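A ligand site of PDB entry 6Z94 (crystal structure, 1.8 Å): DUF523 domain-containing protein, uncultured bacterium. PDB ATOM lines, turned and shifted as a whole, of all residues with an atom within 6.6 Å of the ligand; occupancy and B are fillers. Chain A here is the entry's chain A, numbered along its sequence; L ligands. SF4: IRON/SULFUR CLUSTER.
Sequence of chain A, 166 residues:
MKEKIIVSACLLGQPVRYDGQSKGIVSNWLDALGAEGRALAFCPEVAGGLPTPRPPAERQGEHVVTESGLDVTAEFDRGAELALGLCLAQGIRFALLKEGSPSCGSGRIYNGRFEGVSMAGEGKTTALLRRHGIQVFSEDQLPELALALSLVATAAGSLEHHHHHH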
ATOM      1  N   VAL A   7     -14.909 -14.123 -15.392  1.00  0.00           N
ATOM      2  CA  VAL A   7     -15.566 -15.426 -15.407  1.00  0.00           C
ATOM      3  C   VAL A   7     -16.294 -15.653 -16.715  1.00  0.00           C
ATOM      4  O   VAL A   7     -17.006 -14.750 -17.174  1.00  0.00           O
ATOM      5  CB  VAL A   7     -16.602 -15.539 -14.257  1.00  0.00           C
ATOM      6  CG1 VAL A   7     -17.199 -16.942 -14.168  1.00  0.00           C
ATOM      7  CG2 VAL A   7     -16.004 -15.115 -12.912  1.00  0.00           C
ATOM      8  N   SER A   8     -16.197 -16.891 -17.311  1.00  0.00           N
ATOM      9  CA  SER A   8     -16.936 -17.247 -18.531  1.00  0.00           C
ATOM     10  C   SER A   8     -18.420 -17.008 -18.242  1.00  0.00           C
ATOM     11  O   SER A   8     -18.909 -17.463 -17.196  1.00  0.00           O
ATOM     12  CB  SER A   8     -16.754 -18.722 -18.871  1.00  0.00           C
ATOM     13  OG  SER A   8     -15.496 -18.982 -19.474  1.00  0.00           O
ATOM     14  N   ALA A   9     -19.060 -16.147 -19.043  1.00  0.00           N
ATOM     15  CA  ALA A   9     -20.445 -15.737 -18.853  1.00  0.00           C
ATOM     16  C   ALA A   9     -21.402 -16.920 -18.728  1.00  0.00           C
ATOM     17  O   ALA A   9     -22.351 -16.855 -17.933  1.00  0.00           O
ATOM     18  CB  ALA A   9     -20.883 -14.800 -19.983  1.00  0.00           C
ATOM     19  N   CYS A  10     -21.137 -18.015 -19.451  1.00  0.00           N
ATOM     20  CA  CYS A  10     -21.967 -19.218 -19.371  1.00  0.00           C
ATOM     21  C   CYS A  10     -21.911 -19.828 -17.953  1.00  0.00           C
ATOM     22  O   CYS A  10     -22.929 -20.309 -17.473  1.00  0.00           O
ATOM     23  CB  CYS A  10     -21.561 -20.236 -20.440  1.00  0.00           C
ATOM     24  SG  CYS A  10     -19.829 -20.770 -20.327  1.00  0.00           S
ATOM     25  N   LEU A  11     -20.741 -19.786 -17.264  1.00  0.00           N
ATOM     26  CA  LEU A  11     -20.609 -20.313 -15.892  1.00  0.00           C
ATOM     27  C   LEU A  11     -21.500 -19.553 -14.897  1.00  0.00           C
ATOM     28  O   LEU A  11     -21.847 -20.088 -13.856  1.00  0.00           O
ATOM     29  CB  LEU A  11     -19.163 -20.303 -15.393  1.00  0.00           C
ATOM     30  CG  LEU A  11     -18.200 -21.231 -16.145  1.00  0.00           C
ATOM     31  CD1 LEU A  11     -16.756 -21.021 -15.652  1.00  0.00           C
ATOM     32  CD2 LEU A  11     -18.619 -22.709 -15.991  1.00  0.00           C
ATOM     33  N   GLN A  14     -25.500 -17.334 -17.986  1.00  0.00           N
ATOM     34  CA  GLN A  14     -25.890 -16.574 -19.175  1.00  0.00           C
ATOM     35  C   GLN A  14     -26.061 -17.437 -20.400  1.00  0.00           C
ATOM     36  O   GLN A  14     -25.255 -18.339 -20.628  1.00  0.00           O
ATOM     37  CB  GLN A  14     -24.941 -15.430 -19.413  1.00  0.00           C
ATOM     38  CG  GLN A  14     -24.925 -14.500 -18.219  1.00  0.00           C
ATOM     39  CD  GLN A  14     -24.223 -13.225 -18.505  1.00  0.00           C
ATOM     40  OE1 GLN A  14     -24.083 -12.799 -19.652  1.00  0.00           O
ATOM     41  NE2 GLN A  14     -23.772 -12.569 -17.453  1.00  0.00           N
ATOM     42  N   VAL A  16     -25.309 -17.743 -23.474  1.00  0.00           N
ATOM     43  CA  VAL A  16     -24.421 -17.360 -24.558  1.00  0.00           C
ATOM     44  C   VAL A  16     -23.646 -18.510 -25.196  1.00  0.00           C
ATOM     45  O   VAL A  16     -22.840 -18.252 -26.082  1.00  0.00           O
ATOM     46  CB  VAL A  16     -23.442 -16.272 -24.069  1.00  0.00           C
ATOM     47  CG1 VAL A  16     -24.192 -14.961 -23.828  1.00  0.00           C
ATOM     48  CG2 VAL A  16     -22.698 -16.738 -22.808  1.00  0.00           C
ATOM     49  N   ARG A  17     -23.865 -19.767 -24.764  1.00  0.00           N
ATOM     50  CA  ARG A  17     -23.167 -20.909 -25.367  1.00  0.00           C
ATOM     51  C   ARG A  17     -23.550 -21.021 -26.847  1.00  0.00           C
ATOM     52  O   ARG A  17     -24.576 -20.458 -27.270  1.00  0.00           O
ATOM     53  CB  ARG A  17     -23.561 -22.209 -24.639  1.00  0.00           C
ATOM     54  CG  ARG A  17     -22.961 -22.347 -23.238  1.00  0.00           C
ATOM     55  CD  ARG A  17     -21.522 -22.830 -23.278  1.00  0.00           C
ATOM     56  NE  ARG A  17     -21.454 -24.247 -23.651  1.00  0.00           N
ATOM     57  CZ  ARG A  17     -20.324 -24.962 -23.683  1.00  0.00           C
ATOM     58  NH1 ARG A  17     -19.169 -24.404 -23.341  1.00  0.00           N
ATOM     59  NH2 ARG A  17     -20.357 -26.241 -24.043  1.00  0.00           N
ATOM     60  N   TYR A  18     -22.783 -21.772 -27.645  1.00  0.00           N
ATOM     61  CA  TYR A  18     -23.070 -21.943 -29.060  1.00  0.00           C
ATOM     62  C   TYR A  18     -24.512 -22.428 -29.340  1.00  0.00           C
ATOM     63  O   TYR A  18     -25.055 -22.137 -30.396  1.00  0.00           O
ATOM     64  CB  TYR A  18     -22.048 -22.874 -29.708  1.00  0.00           C
ATOM     65  CG  TYR A  18     -22.296 -24.346 -29.432  1.00  0.00           C
ATOM     66  CD1 TYR A  18     -22.025 -24.904 -28.198  1.00  0.00           C
ATOM     67  CD2 TYR A  18     -22.859 -25.161 -30.410  1.00  0.00           C
ATOM     68  CE1 TYR A  18     -22.277 -26.243 -27.936  1.00  0.00           C
ATOM     69  CE2 TYR A  18     -23.111 -26.516 -30.164  1.00  0.00           C
ATOM     70  CZ  TYR A  18     -22.820 -27.049 -28.919  1.00  0.00           C
ATOM     71  OH  TYR A  18     -23.053 -28.371 -28.674  1.00  0.00           O
ATOM     72  N   GLN A  21     -27.690 -22.357 -24.720  1.00  0.00           N
ATOM     73  CA  GLN A  21     -27.891 -22.734 -23.331  1.00  0.00           C
ATOM     74  C   GLN A  21     -26.800 -22.102 -22.426  1.00  0.00           C
ATOM     75  O   GLN A  21     -26.036 -21.229 -22.874  1.00  0.00           O
ATOM     76  CB  GLN A  21     -28.116 -24.257 -23.145  1.00  0.00           C
ATOM     77  CG  GLN A  21     -26.910 -25.149 -23.269  1.00  0.00           C
ATOM     78  CD  GLN A  21     -27.295 -26.629 -23.309  1.00  0.00           C
ATOM     79  OE1 GLN A  21     -28.416 -27.027 -22.976  1.00  0.00           O
ATOM     80  NE2 GLN A  21     -26.365 -27.483 -23.722  1.00  0.00           N
ATOM     81  N   LYS A  23     -24.101 -22.721 -18.803  1.00  0.00           N
ATOM     82  CA  LYS A  23     -23.354 -23.737 -18.063  1.00  0.00           C
ATOM     83  C   LYS A  23     -23.270 -23.281 -16.625  1.00  0.00           C
ATOM     84  O   LYS A  23     -22.187 -23.262 -16.027  1.00  0.00           O
ATOM     85  CB  LYS A  23     -21.958 -23.933 -18.679  1.00  0.00           C
ATOM     86  CG  LYS A  23     -22.001 -24.624 -20.038  1.00  0.00           C
ATOM     87  CD  LYS A  23     -22.577 -26.045 -19.945  1.00  0.00           C
ATOM     88  CE  LYS A  23     -22.548 -26.755 -21.271  1.00  0.00           C
ATOM     89  NZ  LYS A  23     -22.971 -28.173 -21.159  1.00  0.00           N
ATOM     90  N   PHE A  42     -17.882 -12.512 -18.775  1.00  0.00           N
ATOM     91  CA  PHE A  42     -17.292 -12.217 -20.081  1.00  0.00           C
ATOM     92  C   PHE A  42     -17.400 -13.424 -20.959  1.00  0.00           C
ATOM     93  O   PHE A  42     -17.076 -14.524 -20.506  1.00  0.00           O
ATOM     94  CB  PHE A  42     -15.801 -11.799 -19.940  1.00  0.00           C
ATOM     95  CG  PHE A  42     -15.193 -11.324 -21.246  1.00  0.00           C
ATOM     96  CD1 PHE A  42     -14.445 -12.179 -22.038  1.00  0.00           C
ATOM     97  CD2 PHE A  42     -15.409 -10.029 -21.701  1.00  0.00           C
ATOM     98  CE1 PHE A  42     -13.919 -11.748 -23.248  1.00  0.00           C
ATOM     99  CE2 PHE A  42     -14.884  -9.610 -22.917  1.00  0.00           C
ATOM    100  CZ  PHE A  42     -14.143 -10.465 -23.676  1.00  0.00           C
ATOM    101  N   CYS A  43     -17.866 -13.244 -22.195  1.00  0.00           N
ATOM    102  CA  CYS A  43     -17.902 -14.340 -23.159  1.00  0.00           C
ATOM    103  C   CYS A  43     -17.021 -13.922 -24.329  1.00  0.00           C
ATOM    104  O   CYS A  43     -17.397 -13.009 -25.073  1.00  0.00           O
ATOM    105  CB  CYS A  43     -19.312 -14.655 -23.629  1.00  0.00           C
ATOM    106  SG  CYS A  43     -19.359 -15.866 -24.988  1.00  0.00           S
ATOM    107  N   PRO A  44     -15.875 -14.566 -24.525  1.00  0.00           N
ATOM    108  CA  PRO A  44     -14.990 -14.173 -25.644  1.00  0.00           C
ATOM    109  C   PRO A  44     -15.625 -14.304 -27.024  1.00  0.00           C
ATOM    110  O   PRO A  44     -15.358 -13.472 -27.897  1.00  0.00           O
ATOM    111  CB  PRO A  44     -13.800 -15.138 -25.487  1.00  0.00           C
ATOM    112  CG  PRO A  44     -13.846 -15.636 -24.068  1.00  0.00           C
ATOM    113  CD  PRO A  44     -15.300 -15.656 -23.703  1.00  0.00           C
ATOM    114  N   GLU A  45     -16.442 -15.333 -27.239  1.00  0.00           N
ATOM    115  CA  GLU A  45     -17.033 -15.520 -28.571  1.00  0.00           C
ATOM    116  C   GLU A  45     -18.058 -14.450 -28.905  1.00  0.00           C
ATOM    117  O   GLU A  45     -18.048 -13.915 -30.026  1.00  0.00           O
ATOM    118  CB  GLU A  45     -17.550 -16.924 -28.743  1.00  0.00           C
ATOM    119  CG  GLU A  45     -16.355 -17.853 -28.759  1.00  0.00           C
ATOM    120  CD  GLU A  45     -16.684 -19.317 -28.606  1.00  0.00           C
ATOM    121  OE1 GLU A  45     -17.840 -19.698 -28.924  1.00  0.00           O
ATOM    122  OE2 GLU A  45     -15.804 -20.091 -28.163  1.00  0.00           O
ATOM    123  N   VAL A  46     -18.904 -14.082 -27.915  1.00  0.00           N
ATOM    124  CA  VAL A  46     -19.880 -13.026 -28.142  1.00  0.00           C
ATOM    125  C   VAL A  46     -19.163 -11.663 -28.236  1.00  0.00           C
ATOM    126  O   VAL A  46     -19.469 -10.870 -29.125  1.00  0.00           O
ATOM    127  CB  VAL A  46     -21.004 -13.062 -27.064  1.00  0.00           C
ATOM    128  CG1 VAL A  46     -21.870 -11.835 -27.146  1.00  0.00           C
ATOM    129  CG2 VAL A  46     -21.853 -14.337 -27.223  1.00  0.00           C
ATOM    130  N   ARG A  54     -24.561 -20.325 -32.604  1.00  0.00           N
ATOM    131  CA  ARG A  54     -23.477 -20.336 -33.567  1.00  0.00           C
ATOM    132  C   ARG A  54     -23.009 -21.789 -33.725  1.00  0.00           C
ATOM    133  O   ARG A  54     -23.194 -22.620 -32.827  1.00  0.00           O
ATOM    134  CB  ARG A  54     -22.318 -19.394 -33.125  1.00  0.00           C
ATOM    135  CG  ARG A  54     -21.699 -19.751 -31.776  1.00  0.00           C
ATOM    136  CD  ARG A  54     -20.770 -18.654 -31.286  1.00  0.00           C
ATOM    137  NE  ARG A  54     -20.340 -18.889 -29.900  1.00  0.00           N
ATOM    138  CZ  ARG A  54     -21.028 -18.514 -28.819  1.00  0.00           C
ATOM    139  NH1 ARG A  54     -22.191 -17.878 -28.949  1.00  0.00           N
ATOM    140  NH2 ARG A  54     -20.562 -18.776 -27.608  1.00  0.00           N
ATOM    141  N   PHE A  76     -12.430 -15.222 -32.540  1.00  0.00           N
ATOM    142  CA  PHE A  76     -11.852 -15.862 -31.365  1.00  0.00           C
ATOM    143  C   PHE A  76     -10.684 -15.002 -30.822  1.00  0.00           C
ATOM    144  O   PHE A  76     -10.606 -14.773 -29.613  1.00  0.00           O
ATOM    145  CB  PHE A  76     -11.378 -17.289 -31.693  1.00  0.00           C
ATOM    146  CG  PHE A  76     -12.453 -18.330 -31.512  1.00  0.00           C
ATOM    147  CD1 PHE A  76     -13.566 -18.367 -32.345  1.00  0.00           C
ATOM    148  CD2 PHE A  76     -12.385 -19.251 -30.475  1.00  0.00           C
ATOM    149  CE1 PHE A  76     -14.581 -19.306 -32.151  1.00  0.00           C
ATOM    150  CE2 PHE A  76     -13.391 -20.206 -30.298  1.00  0.00           C
ATOM    151  CZ  PHE A  76     -14.484 -20.221 -31.130  1.00  0.00           C
ATOM    152  N   LEU A  97     -12.632 -19.906 -16.204  1.00  0.00           N
ATOM    153  CA  LEU A  97     -13.132 -20.146 -17.547  1.00  0.00           C
ATOM    154  C   LEU A  97     -13.664 -21.557 -17.768  1.00  0.00           C
ATOM    155  O   LEU A  97     -13.169 -22.511 -17.157  1.00  0.00           O
ATOM    156  CB  LEU A  97     -12.040 -19.771 -18.591  1.00  0.00           C
ATOM    157  CG  LEU A  97     -11.482 -18.330 -18.531  1.00  0.00           C
ATOM    158  CD1 LEU A  97     -10.434 -18.087 -19.643  1.00  0.00           C
ATOM    159  CD2 LEU A  97     -12.598 -17.287 -18.625  1.00  0.00           C
ATOM    160  N   LYS A  98     -14.641 -21.688 -18.676  1.00  0.00           N
ATOM    161  CA  LYS A  98     -15.303 -22.937 -18.996  1.00  0.00           C
ATOM    162  C   LYS A  98     -14.389 -23.984 -19.628  1.00  0.00           C
ATOM    163  O   LYS A  98     -13.776 -23.734 -20.666  1.00  0.00           O
ATOM    164  CB  LYS A  98     -16.545 -22.657 -19.877  1.00  0.00           C
ATOM    165  CG  LYS A  98     -17.279 -23.906 -20.341  1.00  0.00           C
ATOM    166  CD  LYS A  98     -18.035 -24.603 -19.168  1.00  0.00           C
ATOM    167  CE  LYS A  98     -18.455 -26.014 -19.494  1.00  0.00           C
ATOM    168  NZ  LYS A  98     -17.319 -26.987 -19.384  1.00  0.00           N
ATOM    169  N   GLU A  99     -14.313 -25.172 -19.030  1.00  0.00           N
ATOM    170  CA  GLU A  99     -13.479 -26.244 -19.541  1.00  0.00           C
ATOM    171  C   GLU A  99     -13.937 -26.800 -20.914  1.00  0.00           C
ATOM    172  O   GLU A  99     -15.134 -26.829 -21.192  1.00  0.00           O
ATOM    173  CB  GLU A  99     -13.387 -27.387 -18.503  1.00  0.00           C
ATOM    174  CG  GLU A  99     -12.336 -28.438 -18.826  1.00  0.00           C
ATOM    175  CD  GLU A  99     -10.919 -27.904 -18.953  1.00  0.00           C
ATOM    176  OE1 GLU A  99     -10.602 -27.284 -19.990  1.00  0.00           O
ATOM    177  OE2 GLU A  99     -10.106 -28.145 -18.031  1.00  0.00           O
ATOM    178  N   SER A 101     -13.645 -25.706 -23.982  1.00  0.00           N
ATOM    179  CA  SER A 101     -14.005 -24.719 -25.008  1.00  0.00           C
ATOM    180  C   SER A 101     -12.800 -24.319 -25.900  1.00  0.00           C
ATOM    181  O   SER A 101     -11.677 -24.134 -25.405  1.00  0.00           O
ATOM    182  CB  SER A 101     -14.657 -23.500 -24.340  1.00  0.00           C
ATOM    183  OG  SER A 101     -14.709 -22.327 -25.136  1.00  0.00           O
ATOM    184  N   PRO A 102     -13.032 -24.093 -27.213  1.00  0.00           N
ATOM    185  CA  PRO A 102     -11.957 -23.594 -28.076  1.00  0.00           C
ATOM    186  C   PRO A 102     -11.524 -22.157 -27.707  1.00  0.00           C
ATOM    187  O   PRO A 102     -10.486 -21.708 -28.189  1.00  0.00           O
ATOM    188  CB  PRO A 102     -12.565 -23.680 -29.484  1.00  0.00           C
ATOM    189  CG  PRO A 102     -14.025 -23.544 -29.279  1.00  0.00           C
ATOM    190  CD  PRO A 102     -14.317 -24.224 -27.958  1.00  0.00           C
ATOM    191  N   SER A 103     -12.304 -21.447 -26.841  1.00  0.00           N
ATOM    192  CA  SER A 103     -11.984 -20.143 -26.290  1.00  0.00           C
ATOM    193  C   SER A 103     -11.521 -20.261 -24.842  1.00  0.00           C
ATOM    194  O   SER A 103     -10.453 -19.774 -24.479  1.00  0.00           O
ATOM    195  CB  SER A 103     -13.229 -19.247 -26.270  1.00  0.00           C
ATOM    196  OG  SER A 103     -13.503 -18.692 -27.545  1.00  0.00           O
ATOM    197  N   CYS A 104     -12.354 -20.886 -23.975  1.00  0.00           N
ATOM    198  CA  CYS A 104     -12.173 -20.891 -22.533  1.00  0.00           C
ATOM    199  C   CYS A 104     -11.513 -22.130 -21.911  1.00  0.00           C
ATOM    200  O   CYS A 104     -11.184 -22.100 -20.726  1.00  0.00           O
ATOM    201  CB  CYS A 104     -13.539 -20.612 -21.896  1.00  0.00           C
ATOM    202  SG  CYS A 104     -14.263 -19.021 -22.382  1.00  0.00           S
ATOM    203  N   GLY A 105     -11.322 -23.202 -22.679  1.00  0.00           N
ATOM    204  CA  GLY A 105     -10.702 -24.434 -22.182  1.00  0.00           C
ATOM    205  C   GLY A 105      -9.347 -24.186 -21.536  1.00  0.00           C
ATOM    206  O   GLY A 105      -8.652 -23.257 -21.967  1.00  0.00           O
HETATM  207 FE1  SF4 L   1     -18.338 -20.418 -24.898  1.00  0.00          FE
HETATM  208 FE2  SF4 L   1     -18.914 -19.901 -22.219  1.00  0.00          FE
HETATM  209 FE3  SF4 L   1     -18.642 -17.797 -24.044  1.00  0.00          FE
HETATM  210 FE4  SF4 L   1     -16.416 -19.291 -23.212  1.00  0.00          FE
HETATM  211  S1  SF4 L   1     -17.761 -17.895 -21.914  1.00  0.00           S
HETATM  212  S2  SF4 L   1     -16.938 -18.639 -25.404  1.00  0.00           S
HETATM  213  S3  SF4 L   1     -17.347 -21.399 -23.043  1.00  0.00           S
HETATM  214  S4  SF4 L   1     -20.266 -19.440 -24.035  1.00  0.00           S
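The side-chain sulfur of Cys 43 sits close to the backbone NH of Glu 45. SG of Cys 43 lies close to N of Val 46. N of Cys 104 is in hydrogen-bond range of OG of Ser 101, at 3.0 Å. OE2 of Glu 45 is in hydrogen-bond range of OG of Ser 103. N of Lys 98 lies within hydrogen-bond range of OG of Ser 8, 2.9 Å away. The guanidinium group (NH2) of Arg 54 is in hydrogen-bond range of the backbone carbonyl oxygen (O) of Val 16 (2.8 Å). N of Arg 54 sits at hydrogen-bond distance from O of Tyr 18 (2.9 Å). The backbone carbonyl oxygen of Val 7 lies within hydrogen-bond range of the backbone NH of Phe 42, 2.9 Å away.
The side-chain sulfur (SG) of Cys 43 is bound to an iron atom (FE3) of the ligand (2.3 Å). SG of Cys 10 binds FE2 of the ligand (2.3 Å). FE4 of the ligand is bound by SG of Cys 104 (2.3 Å). The side-chain hydroxyl of Ser 8 sits close to a sulfur (S1) of the ligand (3.5 Å). OG of Ser 101 lies close to S3 of the ligand (3.5 Å). A sulfur (S4) of the ligand sits close to the backbone NH (N) of Arg 17 (3.7 Å). NH1 of Arg 17 lies close to S3 of the ligand (3.5 Å). A sulfur (S1) of the ligand sits close to the backbone NH of Ala 9 (3.6 Å). NH2 of Arg 54 sits close to S4 of the ligand, at 3.6 Å.
A sulfur (S4) of the ligand sits close to the backbone carbonyl oxygen (O) of Val 16 (3.5 Å). S1 of the ligand sits close to O of Phe 42, 3.7 Å away. S2 of the ligand lies close to OE2 of Glu 45. Pro 44 touches the ligand (CD to S1, 3.8 Å). CB of Lys 98 touches S3 of the ligand (3.5 Å). CB of Ser 103 touches S2 of the ligand, at 3.9 Å.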
